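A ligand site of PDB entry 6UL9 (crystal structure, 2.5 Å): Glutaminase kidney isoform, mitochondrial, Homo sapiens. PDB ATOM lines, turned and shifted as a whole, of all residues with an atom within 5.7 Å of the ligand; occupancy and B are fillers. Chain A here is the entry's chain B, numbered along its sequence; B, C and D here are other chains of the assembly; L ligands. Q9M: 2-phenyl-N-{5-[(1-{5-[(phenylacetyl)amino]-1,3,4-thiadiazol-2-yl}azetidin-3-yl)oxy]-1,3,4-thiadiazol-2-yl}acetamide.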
ATOM      1  N   ARG A 246     -24.141 -20.141   4.123  1.00  0.00           N
ATOM      2  CA  ARG A 246     -24.044 -21.605   4.030  1.00  0.00           C
ATOM      3  C   ARG A 246     -23.065 -22.109   5.069  1.00  0.00           C
ATOM      4  O   ARG A 246     -22.148 -22.895   4.794  1.00  0.00           O
ATOM      5  CB  ARG A 246     -23.704 -22.115   2.624  1.00  0.00           C
ATOM      6  CG  ARG A 246     -24.257 -23.536   2.393  1.00  0.00           C
ATOM      7  CD  ARG A 246     -23.769 -24.146   1.100  1.00  0.00           C
ATOM      8  NE  ARG A 246     -22.363 -24.520   1.155  1.00  0.00           N
ATOM      9  CZ  ARG A 246     -21.356 -23.714   0.841  1.00  0.00           C
ATOM     10  NH1 ARG A 246     -21.579 -22.512   0.329  1.00  0.00           N
ATOM     11  NH2 ARG A 246     -20.104 -24.152   0.937  1.00  0.00           N
ATOM     12  N   PHE A 247     -23.321 -21.695   6.303  1.00  0.00           N
ATOM     13  CA  PHE A 247     -23.186 -22.548   7.462  1.00  0.00           C
ATOM     14  C   PHE A 247     -24.588 -22.859   7.984  1.00  0.00           C
ATOM     15  O   PHE A 247     -24.759 -23.382   9.089  1.00  0.00           O
ATOM     16  CB  PHE A 247     -22.305 -21.875   8.532  1.00  0.00           C
ATOM     17  CG  PHE A 247     -20.808 -21.959   8.250  1.00  0.00           C
ATOM     18  CD1 PHE A 247     -20.285 -22.942   7.422  1.00  0.00           C
ATOM     19  CD2 PHE A 247     -19.931 -21.039   8.816  1.00  0.00           C
ATOM     20  CE1 PHE A 247     -18.909 -23.017   7.175  1.00  0.00           C
ATOM     21  CE2 PHE A 247     -18.554 -21.100   8.569  1.00  0.00           C
ATOM     22  CZ  PHE A 247     -18.050 -22.095   7.741  1.00  0.00           C
ATOM     23  N   LYS A 249     -26.437 -25.132   6.762  1.00  0.00           N
ATOM     24  CA  LYS A 249     -26.595 -26.585   6.660  1.00  0.00           C
ATOM     25  C   LYS A 249     -25.967 -27.316   7.829  1.00  0.00           C
ATOM     26  O   LYS A 249     -26.197 -28.523   7.970  1.00  0.00           O
ATOM     27  CB  LYS A 249     -25.970 -27.085   5.365  1.00  0.00           C
ATOM     28  CG  LYS A 249     -26.791 -26.866   4.118  1.00  0.00           C
ATOM     29  CD  LYS A 249     -25.908 -26.941   2.876  1.00  0.00           C
ATOM     30  CE  LYS A 249     -26.731 -27.145   1.609  1.00  0.00           C
ATOM     31  NZ  LYS A 249     -25.867 -27.401   0.406  1.00  0.00           N
ATOM     32  N   LEU A 250     -25.161 -26.635   8.648  1.00  0.00           N
ATOM     33  CA  LEU A 250     -24.533 -27.224   9.812  1.00  0.00           C
ATOM     34  C   LEU A 250     -25.444 -27.146  11.038  1.00  0.00           C
ATOM     35  O   LEU A 250     -26.145 -26.147  11.251  1.00  0.00           O
ATOM     36  CB  LEU A 250     -23.224 -26.513  10.123  1.00  0.00           C
ATOM     37  CG  LEU A 250     -22.300 -26.400   8.910  1.00  0.00           C
ATOM     38  CD1 LEU A 250     -20.938 -25.933   9.354  1.00  0.00           C
ATOM     39  CD2 LEU A 250     -22.237 -27.734   8.170  1.00  0.00           C
ATOM     40  N   PHE A 251     -25.412 -28.212  11.844  1.00  0.00           N
ATOM     41  CA  PHE A 251     -26.229 -28.268  13.047  1.00  0.00           C
ATOM     42  C   PHE A 251     -25.606 -27.508  14.212  1.00  0.00           C
ATOM     43  O   PHE A 251     -26.333 -26.975  15.059  1.00  0.00           O
ATOM     44  CB  PHE A 251     -26.427 -29.733  13.456  1.00  0.00           C
ATOM     45  CG  PHE A 251     -27.069 -30.580  12.397  1.00  0.00           C
ATOM     46  CD1 PHE A 251     -27.747 -29.995  11.338  1.00  0.00           C
ATOM     47  CD2 PHE A 251     -27.004 -31.949  12.463  1.00  0.00           C
ATOM     48  CE1 PHE A 251     -28.334 -30.760  10.366  1.00  0.00           C
ATOM     49  CE2 PHE A 251     -27.604 -32.727  11.499  1.00  0.00           C
ATOM     50  CZ  PHE A 251     -28.274 -32.128  10.449  1.00  0.00           C
ATOM     51  N   LEU A 252     -24.275 -27.430  14.257  1.00  0.00           N
ATOM     52  CA  LEU A 252     -23.571 -26.860  15.394  1.00  0.00           C
ATOM     53  C   LEU A 252     -22.550 -25.848  14.900  1.00  0.00           C
ATOM     54  O   LEU A 252     -21.995 -25.996  13.815  1.00  0.00           O
ATOM     55  CB  LEU A 252     -22.864 -27.928  16.226  1.00  0.00           C
ATOM     56  CG  LEU A 252     -23.799 -28.991  16.780  1.00  0.00           C
ATOM     57  CD1 LEU A 252     -23.016 -30.056  17.572  1.00  0.00           C
ATOM     58  CD2 LEU A 252     -24.863 -28.307  17.645  1.00  0.00           C
ATOM     59  N   ASN A 253     -22.317 -24.821  15.714  1.00  0.00           N
ATOM     60  CA  ASN A 253     -21.220 -23.903  15.466  1.00  0.00           C
ATOM     61  C   ASN A 253     -19.915 -24.540  15.975  1.00  0.00           C
ATOM     62  O   ASN A 253     -19.861 -25.736  16.251  1.00  0.00           O
ATOM     63  CB  ASN A 253     -21.510 -22.543  16.095  1.00  0.00           C
ATOM     64  CG  ASN A 253     -21.534 -22.584  17.633  1.00  0.00           C
ATOM     65  OD1 ASN A 253     -21.008 -23.507  18.269  1.00  0.00           O
ATOM     66  ND2 ASN A 253     -22.176 -21.565  18.230  1.00  0.00           N
ATOM     67  N   GLU A 254     -18.859 -23.738  16.111  1.00  0.00           N
ATOM     68  CA  GLU A 254     -17.578 -24.313  16.483  1.00  0.00           C
ATOM     69  C   GLU A 254     -17.497 -24.676  17.957  1.00  0.00           C
ATOM     70  O   GLU A 254     -16.702 -25.537  18.329  1.00  0.00           O
ATOM     71  CB  GLU A 254     -16.449 -23.338  16.131  1.00  0.00           C
ATOM     72  CG  GLU A 254     -16.475 -22.903  14.684  1.00  0.00           C
ATOM     73  CD  GLU A 254     -15.236 -22.131  14.260  1.00  0.00           C
ATOM     74  OE1 GLU A 254     -14.236 -22.113  15.021  1.00  0.00           O
ATOM     75  OE2 GLU A 254     -15.255 -21.548  13.154  1.00  0.00           O
ATOM     76  N   ASP A 255     -18.338 -24.072  18.800  1.00  0.00           N
ATOM     77  CA  ASP A 255     -18.401 -24.433  20.214  1.00  0.00           C
ATOM     78  C   ASP A 255     -19.353 -25.583  20.473  1.00  0.00           C
ATOM     79  O   ASP A 255     -19.747 -25.797  21.624  1.00  0.00           O
ATOM     80  CB  ASP A 255     -18.837 -23.225  21.056  1.00  0.00           C
ATOM     81  CG  ASP A 255     -18.046 -21.976  20.754  1.00  0.00           C
ATOM     82  OD1 ASP A 255     -16.821 -22.088  20.498  1.00  0.00           O
ATOM     83  OD2 ASP A 255     -18.651 -20.890  20.773  1.00  0.00           O
ATOM     84  N   ASP A 256     -19.743 -26.320  19.429  1.00  0.00           N
ATOM     85  CA  ASP A 256     -20.608 -27.494  19.556  1.00  0.00           C
ATOM     86  C   ASP A 256     -21.964 -27.166  20.177  1.00  0.00           C
ATOM     87  O   ASP A 256     -22.619 -28.045  20.732  1.00  0.00           O
ATOM     88  CB  ASP A 256     -19.918 -28.604  20.348  1.00  0.00           C
ATOM     89  CG  ASP A 256     -18.904 -29.352  19.526  1.00  0.00           C
ATOM     90  OD1 ASP A 256     -18.952 -29.241  18.283  1.00  0.00           O
ATOM     91  OD2 ASP A 256     -18.064 -30.060  20.117  1.00  0.00           O
ATOM     92  N   HIS A 259     -26.434 -22.778  16.494  1.00  0.00           N
ATOM     93  CA  HIS A 259     -25.984 -21.410  16.272  1.00  0.00           C
ATOM     94  C   HIS A 259     -26.844 -20.428  17.039  1.00  0.00           C
ATOM     95  O   HIS A 259     -26.342 -19.439  17.584  1.00  0.00           O
ATOM     96  CB  HIS A 259     -26.022 -21.075  14.779  1.00  0.00           C
ATOM     97  CG  HIS A 259     -25.244 -22.027  13.949  1.00  0.00           C
ATOM     98  ND1 HIS A 259     -23.915 -21.841  13.651  1.00  0.00           N
ATOM     99  CD2 HIS A 259     -25.597 -23.214  13.401  1.00  0.00           C
ATOM    100  CE1 HIS A 259     -23.480 -22.858  12.940  1.00  0.00           C
ATOM    101  NE2 HIS A 259     -24.478 -23.705  12.762  1.00  0.00           N
ATOM    102  N   TYR A 323     -27.652 -36.269  16.317  1.00  0.00           N
ATOM    103  CA  TYR A 323     -26.411 -35.505  16.265  1.00  0.00           C
ATOM    104  C   TYR A 323     -26.191 -34.695  17.549  1.00  0.00           C
ATOM    105  O   TYR A 323     -25.058 -34.639  18.054  1.00  0.00           O
ATOM    106  CB  TYR A 323     -26.457 -34.566  15.064  1.00  0.00           C
ATOM    107  CG  TYR A 323     -25.101 -34.043  14.680  1.00  0.00           C
ATOM    108  CD1 TYR A 323     -24.600 -32.881  15.259  1.00  0.00           C
ATOM    109  CD2 TYR A 323     -24.329 -34.700  13.723  1.00  0.00           C
ATOM    110  CE1 TYR A 323     -23.344 -32.409  14.904  1.00  0.00           C
ATOM    111  CE2 TYR A 323     -23.078 -34.227  13.360  1.00  0.00           C
ATOM    112  CZ  TYR A 323     -22.591 -33.077  13.948  1.00  0.00           C
ATOM    113  OH  TYR A 323     -21.352 -32.603  13.592  1.00  0.00           O
ATOM    114  N   ARG B 246     -10.964 -30.610   6.052  1.00  0.00           N
ATOM    115  CA  ARG B 246     -12.123 -30.350   6.887  1.00  0.00           C
ATOM    116  C   ARG B 246     -13.369 -30.212   6.010  1.00  0.00           C
ATOM    117  O   ARG B 246     -14.078 -29.213   6.022  1.00  0.00           O
ATOM    118  CB  ARG B 246     -11.925 -29.137   7.796  1.00  0.00           C
ATOM    119  CG  ARG B 246     -12.919 -29.086   8.943  1.00  0.00           C
ATOM    120  CD  ARG B 246     -12.836 -27.824   9.787  1.00  0.00           C
ATOM    121  NE  ARG B 246     -12.762 -26.615   8.977  1.00  0.00           N
ATOM    122  CZ  ARG B 246     -13.784 -26.063   8.320  1.00  0.00           C
ATOM    123  NH1 ARG B 246     -14.963 -26.675   8.265  1.00  0.00           N
ATOM    124  NH2 ARG B 246     -13.602 -24.950   7.614  1.00  0.00           N
ATOM    125  N   PHE B 247     -13.596 -31.241   5.180  1.00  0.00           N
ATOM    126  CA  PHE B 247     -14.935 -31.733   4.877  1.00  0.00           C
ATOM    127  C   PHE B 247     -15.094 -33.132   5.468  1.00  0.00           C
ATOM    128  O   PHE B 247     -16.049 -33.855   5.134  1.00  0.00           O
ATOM    129  CB  PHE B 247     -15.178 -31.721   3.373  1.00  0.00           C
ATOM    130  CG  PHE B 247     -15.492 -30.366   2.822  1.00  0.00           C
ATOM    131  CD1 PHE B 247     -16.117 -29.413   3.610  1.00  0.00           C
ATOM    132  CD2 PHE B 247     -15.160 -30.029   1.514  1.00  0.00           C
ATOM    133  CE1 PHE B 247     -16.437 -28.142   3.094  1.00  0.00           C
ATOM    134  CE2 PHE B 247     -15.470 -28.773   0.992  1.00  0.00           C
ATOM    135  CZ  PHE B 247     -16.113 -27.818   1.779  1.00  0.00           C
ATOM    136  N   LYS B 249     -16.069 -33.716   8.262  1.00  0.00           N
ATOM    137  CA  LYS B 249     -17.212 -33.549   9.154  1.00  0.00           C
ATOM    138  C   LYS B 249     -18.568 -33.561   8.453  1.00  0.00           C
ATOM    139  O   LYS B 249     -19.583 -33.782   9.128  1.00  0.00           O
ATOM    140  CB  LYS B 249     -17.056 -32.227   9.939  1.00  0.00           C
ATOM    141  CG  LYS B 249     -16.028 -32.222  11.008  1.00  0.00           C
ATOM    142  CD  LYS B 249     -16.332 -31.384  12.165  1.00  0.00           C
ATOM    143  CE  LYS B 249     -16.313 -32.461  13.220  1.00  0.00           C
ATOM    144  NZ  LYS B 249     -17.254 -33.448  13.117  1.00  0.00           N
ATOM    145  N   LEU B 250     -18.634 -33.373   7.129  1.00  0.00           N
ATOM    146  CA  LEU B 250     -19.894 -33.413   6.397  1.00  0.00           C
ATOM    147  C   LEU B 250     -20.259 -34.851   5.989  1.00  0.00           C
ATOM    148  O   LEU B 250     -19.386 -35.661   5.682  1.00  0.00           O
ATOM    149  CB  LEU B 250     -19.835 -32.518   5.158  1.00  0.00           C
ATOM    150  CG  LEU B 250     -19.523 -31.024   5.350  1.00  0.00           C
ATOM    151  CD1 LEU B 250     -19.875 -30.254   4.081  1.00  0.00           C
ATOM    152  CD2 LEU B 250     -20.232 -30.431   6.550  1.00  0.00           C
ATOM    153  N   PHE B 251     -21.566 -35.171   6.035  1.00  0.00           N
ATOM    154  CA  PHE B 251     -22.027 -36.495   5.638  1.00  0.00           C
ATOM    155  C   PHE B 251     -22.120 -36.638   4.122  1.00  0.00           C
ATOM    156  O   PHE B 251     -22.052 -37.758   3.607  1.00  0.00           O
ATOM    157  CB  PHE B 251     -23.403 -36.822   6.227  1.00  0.00           C
ATOM    158  CG  PHE B 251     -23.474 -36.744   7.718  1.00  0.00           C
ATOM    159  CD1 PHE B 251     -22.337 -36.836   8.491  1.00  0.00           C
ATOM    160  CD2 PHE B 251     -24.692 -36.569   8.335  1.00  0.00           C
ATOM    161  CE1 PHE B 251     -22.411 -36.754   9.863  1.00  0.00           C
ATOM    162  CE2 PHE B 251     -24.786 -36.500   9.708  1.00  0.00           C
ATOM    163  CZ  PHE B 251     -23.642 -36.585  10.476  1.00  0.00           C
ATOM    164  N   LEU B 252     -22.352 -35.528   3.418  1.00  0.00           N
ATOM    165  CA  LEU B 252     -22.639 -35.528   1.992  1.00  0.00           C
ATOM    166  C   LEU B 252     -21.747 -34.508   1.284  1.00  0.00           C
ATOM    167  O   LEU B 252     -21.408 -33.468   1.857  1.00  0.00           O
ATOM    168  CB  LEU B 252     -24.100 -35.205   1.729  1.00  0.00           C
ATOM    169  CG  LEU B 252     -25.180 -36.074   2.380  1.00  0.00           C
ATOM    170  CD1 LEU B 252     -26.528 -35.580   1.929  1.00  0.00           C
ATOM    171  CD2 LEU B 252     -25.012 -37.531   1.985  1.00  0.00           C
ATOM    172  N   ASN B 253     -21.361 -34.817   0.051  1.00  0.00           N
ATOM    173  CA  ASN B 253     -20.732 -33.825  -0.807  1.00  0.00           C
ATOM    174  C   ASN B 253     -21.845 -32.981  -1.424  1.00  0.00           C
ATOM    175  O   ASN B 253     -23.015 -33.107  -1.049  1.00  0.00           O
ATOM    176  CB  ASN B 253     -19.819 -34.531  -1.825  1.00  0.00           C
ATOM    177  CG  ASN B 253     -20.584 -35.451  -2.782  1.00  0.00           C
ATOM    178  OD1 ASN B 253     -21.800 -35.334  -2.955  1.00  0.00           O
ATOM    179  ND2 ASN B 253     -19.848 -36.383  -3.413  1.00  0.00           N
ATOM    180  N   GLU B 254     -21.540 -32.086  -2.394  1.00  0.00           N
ATOM    181  CA  GLU B 254     -22.665 -31.324  -2.934  1.00  0.00           C
ATOM    182  C   GLU B 254     -23.536 -32.040  -3.953  1.00  0.00           C
ATOM    183  O   GLU B 254     -24.579 -31.474  -4.317  1.00  0.00           O
ATOM    184  CB  GLU B 254     -22.381 -29.888  -3.439  1.00  0.00           C
ATOM    185  CG  GLU B 254     -21.385 -29.007  -2.715  1.00  0.00           C
ATOM    186  CD  GLU B 254     -20.769 -27.941  -3.560  1.00  0.00           C
ATOM    187  OE1 GLU B 254     -21.542 -27.110  -4.081  1.00  0.00           O
ATOM    188  OE2 GLU B 254     -19.535 -27.697  -3.404  1.00  0.00           O
ATOM    189  N   ASP B 256     -25.052 -34.458  -2.918  1.00  0.00           N
ATOM    190  CA  ASP B 256     -25.866 -35.099  -1.892  1.00  0.00           C
ATOM    191  C   ASP B 256     -25.615 -36.607  -1.826  1.00  0.00           C
ATOM    192  O   ASP B 256     -26.481 -37.393  -1.449  1.00  0.00           O
ATOM    193  CB  ASP B 256     -27.344 -34.764  -2.094  1.00  0.00           C
ATOM    194  CG  ASP B 256     -27.698 -33.371  -1.565  1.00  0.00           C
ATOM    195  OD1 ASP B 256     -27.004 -32.865  -0.655  1.00  0.00           O
ATOM    196  OD2 ASP B 256     -28.678 -32.791  -2.067  1.00  0.00           O
ATOM    197  N   TYR B 323     -30.122 -38.548   8.417  1.00  0.00           N
ATOM    198  CA  TYR B 323     -29.722 -37.544   7.424  1.00  0.00           C
ATOM    199  C   TYR B 323     -29.767 -38.111   6.011  1.00  0.00           C
ATOM    200  O   TYR B 323     -30.233 -37.442   5.080  1.00  0.00           O
ATOM    201  CB  TYR B 323     -28.330 -37.001   7.743  1.00  0.00           C
ATOM    202  CG  TYR B 323     -28.037 -35.701   7.055  1.00  0.00           C
ATOM    203  CD1 TYR B 323     -28.519 -34.500   7.554  1.00  0.00           C
ATOM    204  CD2 TYR B 323     -27.291 -35.656   5.888  1.00  0.00           C
ATOM    205  CE1 TYR B 323     -28.262 -33.286   6.922  1.00  0.00           C
ATOM    206  CE2 TYR B 323     -27.018 -34.452   5.245  1.00  0.00           C
ATOM    207  CZ  TYR B 323     -27.503 -33.271   5.756  1.00  0.00           C
ATOM    208  OH  TYR B 323     -27.243 -32.080   5.122  1.00  0.00           O
ATOM    209  N   LYS B 327     -32.339 -37.006   2.867  1.00  0.00           N
ATOM    210  CA  LYS B 327     -31.713 -36.591   1.618  1.00  0.00           C
ATOM    211  C   LYS B 327     -31.818 -37.651   0.533  1.00  0.00           C
ATOM    212  O   LYS B 327     -31.226 -37.468  -0.536  1.00  0.00           O
ATOM    213  CB  LYS B 327     -30.255 -36.223   1.858  1.00  0.00           C
ATOM    214  CG  LYS B 327     -30.039 -34.864   2.507  1.00  0.00           C
ATOM    215  CD  LYS B 327     -31.102 -33.869   2.118  1.00  0.00           C
ATOM    216  CE  LYS B 327     -30.663 -32.451   2.475  1.00  0.00           C
ATOM    217  NZ  LYS B 327     -29.626 -31.922   1.522  1.00  0.00           N
ATOM    218  N   ARG C 246     -16.925 -18.267  10.490  1.00  0.00           N
ATOM    219  CA  ARG C 246     -15.709 -18.440   9.706  1.00  0.00           C
ATOM    220  C   ARG C 246     -16.020 -18.454   8.223  1.00  0.00           C
ATOM    221  O   ARG C 246     -15.709 -19.399   7.491  1.00  0.00           O
ATOM    222  CB  ARG C 246     -14.827 -19.611  10.099  1.00  0.00           C
ATOM    223  CG  ARG C 246     -13.388 -19.100   9.900  1.00  0.00           C
ATOM    224  CD  ARG C 246     -12.234 -19.841  10.542  1.00  0.00           C
ATOM    225  NE  ARG C 246     -12.231 -21.280  10.406  1.00  0.00           N
ATOM    226  CZ  ARG C 246     -12.425 -22.124  11.412  1.00  0.00           C
ATOM    227  NH1 ARG C 246     -12.564 -21.662  12.642  1.00  0.00           N
ATOM    228  NH2 ARG C 246     -12.404 -23.434  11.185  1.00  0.00           N
ATOM    229  N   ARG D 246     -14.487 -28.238  -3.117  1.00  0.00           N
ATOM    230  CA  ARG D 246     -14.669 -26.797  -2.979  1.00  0.00           C
ATOM    231  C   ARG D 246     -13.949 -26.352  -1.715  1.00  0.00           C
ATOM    232  O   ARG D 246     -14.493 -25.650  -0.851  1.00  0.00           O
ATOM    233  CB  ARG D 246     -16.141 -26.376  -2.976  1.00  0.00           C
ATOM    234  CG  ARG D 246     -16.336 -24.876  -3.249  1.00  0.00           C
ATOM    235  CD  ARG D 246     -17.259 -24.578  -4.422  1.00  0.00           C
ATOM    236  NE  ARG D 246     -17.162 -23.178  -4.826  1.00  0.00           N
ATOM    237  CZ  ARG D 246     -16.502 -22.747  -5.904  1.00  0.00           C
ATOM    238  NH1 ARG D 246     -15.782 -23.589  -6.641  1.00  0.00           N
ATOM    239  NH2 ARG D 246     -16.491 -21.445  -6.182  1.00  0.00           N
HETATM  240  C10 Q9M L   1     -24.092 -32.413   8.809  1.00  0.00           C
HETATM  241  C13 Q9M L   1     -24.280 -32.355   6.606  1.00  0.00           C
HETATM  242  C20 Q9M L   1     -22.412 -29.211   0.522  1.00  0.00           C
HETATM  243  C21 Q9M L   1     -22.593 -27.872   0.206  1.00  0.00           C
HETATM  244  C22 Q9M L   1     -21.478 -27.066   0.061  1.00  0.00           C
HETATM  245  C24 Q9M L   1     -20.021 -28.909   0.538  1.00  0.00           C
HETATM  246  C01 Q9M L   1     -18.165 -26.883  13.966  1.00  0.00           C
HETATM  247  C02 Q9M L   1     -18.996 -27.888  13.184  1.00  0.00           C
HETATM  248  C04 Q9M L   1     -21.015 -29.099  12.469  1.00  0.00           C
HETATM  249  C07 Q9M L   1     -22.341 -30.605  11.029  1.00  0.00           C
HETATM  250  C09 Q9M L   1     -24.511 -32.108  10.197  1.00  0.00           C
HETATM  251  C11 Q9M L   1     -22.858 -31.747   8.793  1.00  0.00           C
HETATM  252  C16 Q9M L   1     -23.584 -31.423   4.345  1.00  0.00           C
HETATM  253  C18 Q9M L   1     -23.968 -30.405   2.131  1.00  0.00           C
HETATM  254  C19 Q9M L   1     -23.612 -30.126   0.683  1.00  0.00           C
HETATM  255  C23 Q9M L   1     -20.185 -27.572   0.222  1.00  0.00           C
HETATM  256  C25 Q9M L   1     -21.132 -29.729   0.692  1.00  0.00           C
HETATM  257  C30 Q9M L   1     -17.678 -25.893  12.926  1.00  0.00           C
HETATM  258  C31 Q9M L   1     -16.344 -25.810  12.534  1.00  0.00           C
HETATM  259  C32 Q9M L   1     -15.960 -24.882  11.572  1.00  0.00           C
HETATM  260  C33 Q9M L   1     -16.881 -24.042  10.971  1.00  0.00           C
HETATM  261  C34 Q9M L   1     -18.216 -24.132  11.351  1.00  0.00           C
HETATM  262  C35 Q9M L   1     -18.600 -25.060  12.313  1.00  0.00           C
HETATM  263  N03 Q9M L   1     -20.401 -28.139  13.385  1.00  0.00           N
HETATM  264  N05 Q9M L   1     -20.354 -29.838  11.597  1.00  0.00           N
HETATM  265  N06 Q9M L   1     -21.063 -30.707  10.847  1.00  0.00           N
HETATM  266  N08 Q9M L   1     -23.209 -31.407  10.197  1.00  0.00           N
HETATM  267  N14 Q9M L   1     -24.546 -31.073   6.381  1.00  0.00           N
HETATM  268  N15 Q9M L   1     -24.175 -30.560   5.153  1.00  0.00           N
HETATM  269  N17 Q9M L   1     -23.104 -31.200   2.991  1.00  0.00           N
HETATM  270  O12 Q9M L   1     -24.614 -33.090   7.761  1.00  0.00           O
HETATM  271  O26 Q9M L   1     -24.969 -29.979   2.578  1.00  0.00           O
HETATM  272  O29 Q9M L   1     -18.429 -28.450  12.323  1.00  0.00           O
HETATM  273  S27 Q9M L   1     -23.521 -32.921   5.168  1.00  0.00           S
HETATM  274  S28 Q9M L   1     -22.669 -29.413  12.208  1.00  0.00           S
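The backbone NH (N) of Leu 252 of chain A sits close to a sulfur (S28) of the ligand (3.3 Å).
The backbone carbonyl oxygen (O) of Leu 252 of chain A lies within hydrogen-bond range of a nitrogen (N03) of the ligand (2.7 Å).
A sulfur (S28) of the ligand sits close to the backbone NH of Phe 251 of chain A.
S27 of the ligand sits close to N of Leu 252 of chain B, 3.4 Å away.
N17 of the ligand sits at hydrogen-bond distance from O of Leu 252 of chain B, at 3.1 Å.
The backbone NH of Phe 251 of chain B sits close to a sulfur (S27) of the ligand, at 3.1 Å.
OH of Tyr 323 of chain B sits at hydrogen-bond distance from N14 of the ligand (3.1 Å).
The side-chain amino group (NZ) of Lys 249 of chain A sits close to an oxygen (O26) of the ligand (3.5 Å).
The side-chain hydroxyl of Tyr 323 of chain A is in hydrogen-bond range of a nitrogen (N06) of the ligand (3.3 Å).
The side-chain amide oxygen of Asn 253 of chain A lies within hydrogen-bond range of the backbone NH of Asp 256 of chain A, 3.3 Å away.
The backbone NH (N) of Asp 255 is in hydrogen-bond range of the side-chain amide oxygen (OD1) of Asn 253 of chain A (2.8 Å).
The backbone NH (N) of Asp 256 of chain B sits at hydrogen-bond distance from the side-chain amide oxygen (OD1) of Asn 253 of chain B (3.4 Å).
O of Leu 250 of chain A is in hydrogen-bond range of NE2 of His 259.
The side-chain carboxylate (OE2) of Glu 254 of chain A lies within salt-bridge range of the guanidinium group (NH1) of Arg 246 of chain C (2.7 Å).
NE of Arg 246 of chain A touches C22 of the ligand, 2.9 Å away.
Phe 247 of chain A touches the ligand (CZ to C33, 3.9 Å).
CB of Leu 250 of chain A touches S28 of the ligand (3.6 Å).
Asn 253 of chain A touches the ligand.
Glu 254 of chain A touches the ligand.
Arg 246 of chain B touches the ligand.
Lys 249 of chain B touches the ligand (CD to O29, 3.6 Å).
CD1 of Leu 250 of chain B touches N17 of the ligand (3.5 Å).
Asn 253 of chain B touches the ligand (O to C19, 3.5 Å).
CG of Glu 254 of chain B touches C21 of the ligand, at 3.4 Å.
Arg 246 of chain C touches the ligand.
18 residues have an atom within 4 Å of the ligand: Arg 246 of chain A, Phe 247 of chain A, Lys 249 of chain A, Leu 250 of chain A, Phe 251 of chain A, Leu 252 of chain A, Asn 253 of chain A, Glu 254 of chain A, Tyr 323 of chain A, Arg 246 of chain B, Lys 249 of chain B, Leu 250 of chain B, Phe 251 of chain B, Leu 252 of chain B, Asn 253 of chain B, Glu 254 of chain B, Tyr 323 of chain B and Arg 246 of chain C.
The nearest printed residue that does not touch the ligand is Phe 247 of chain B (4.2 Å).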
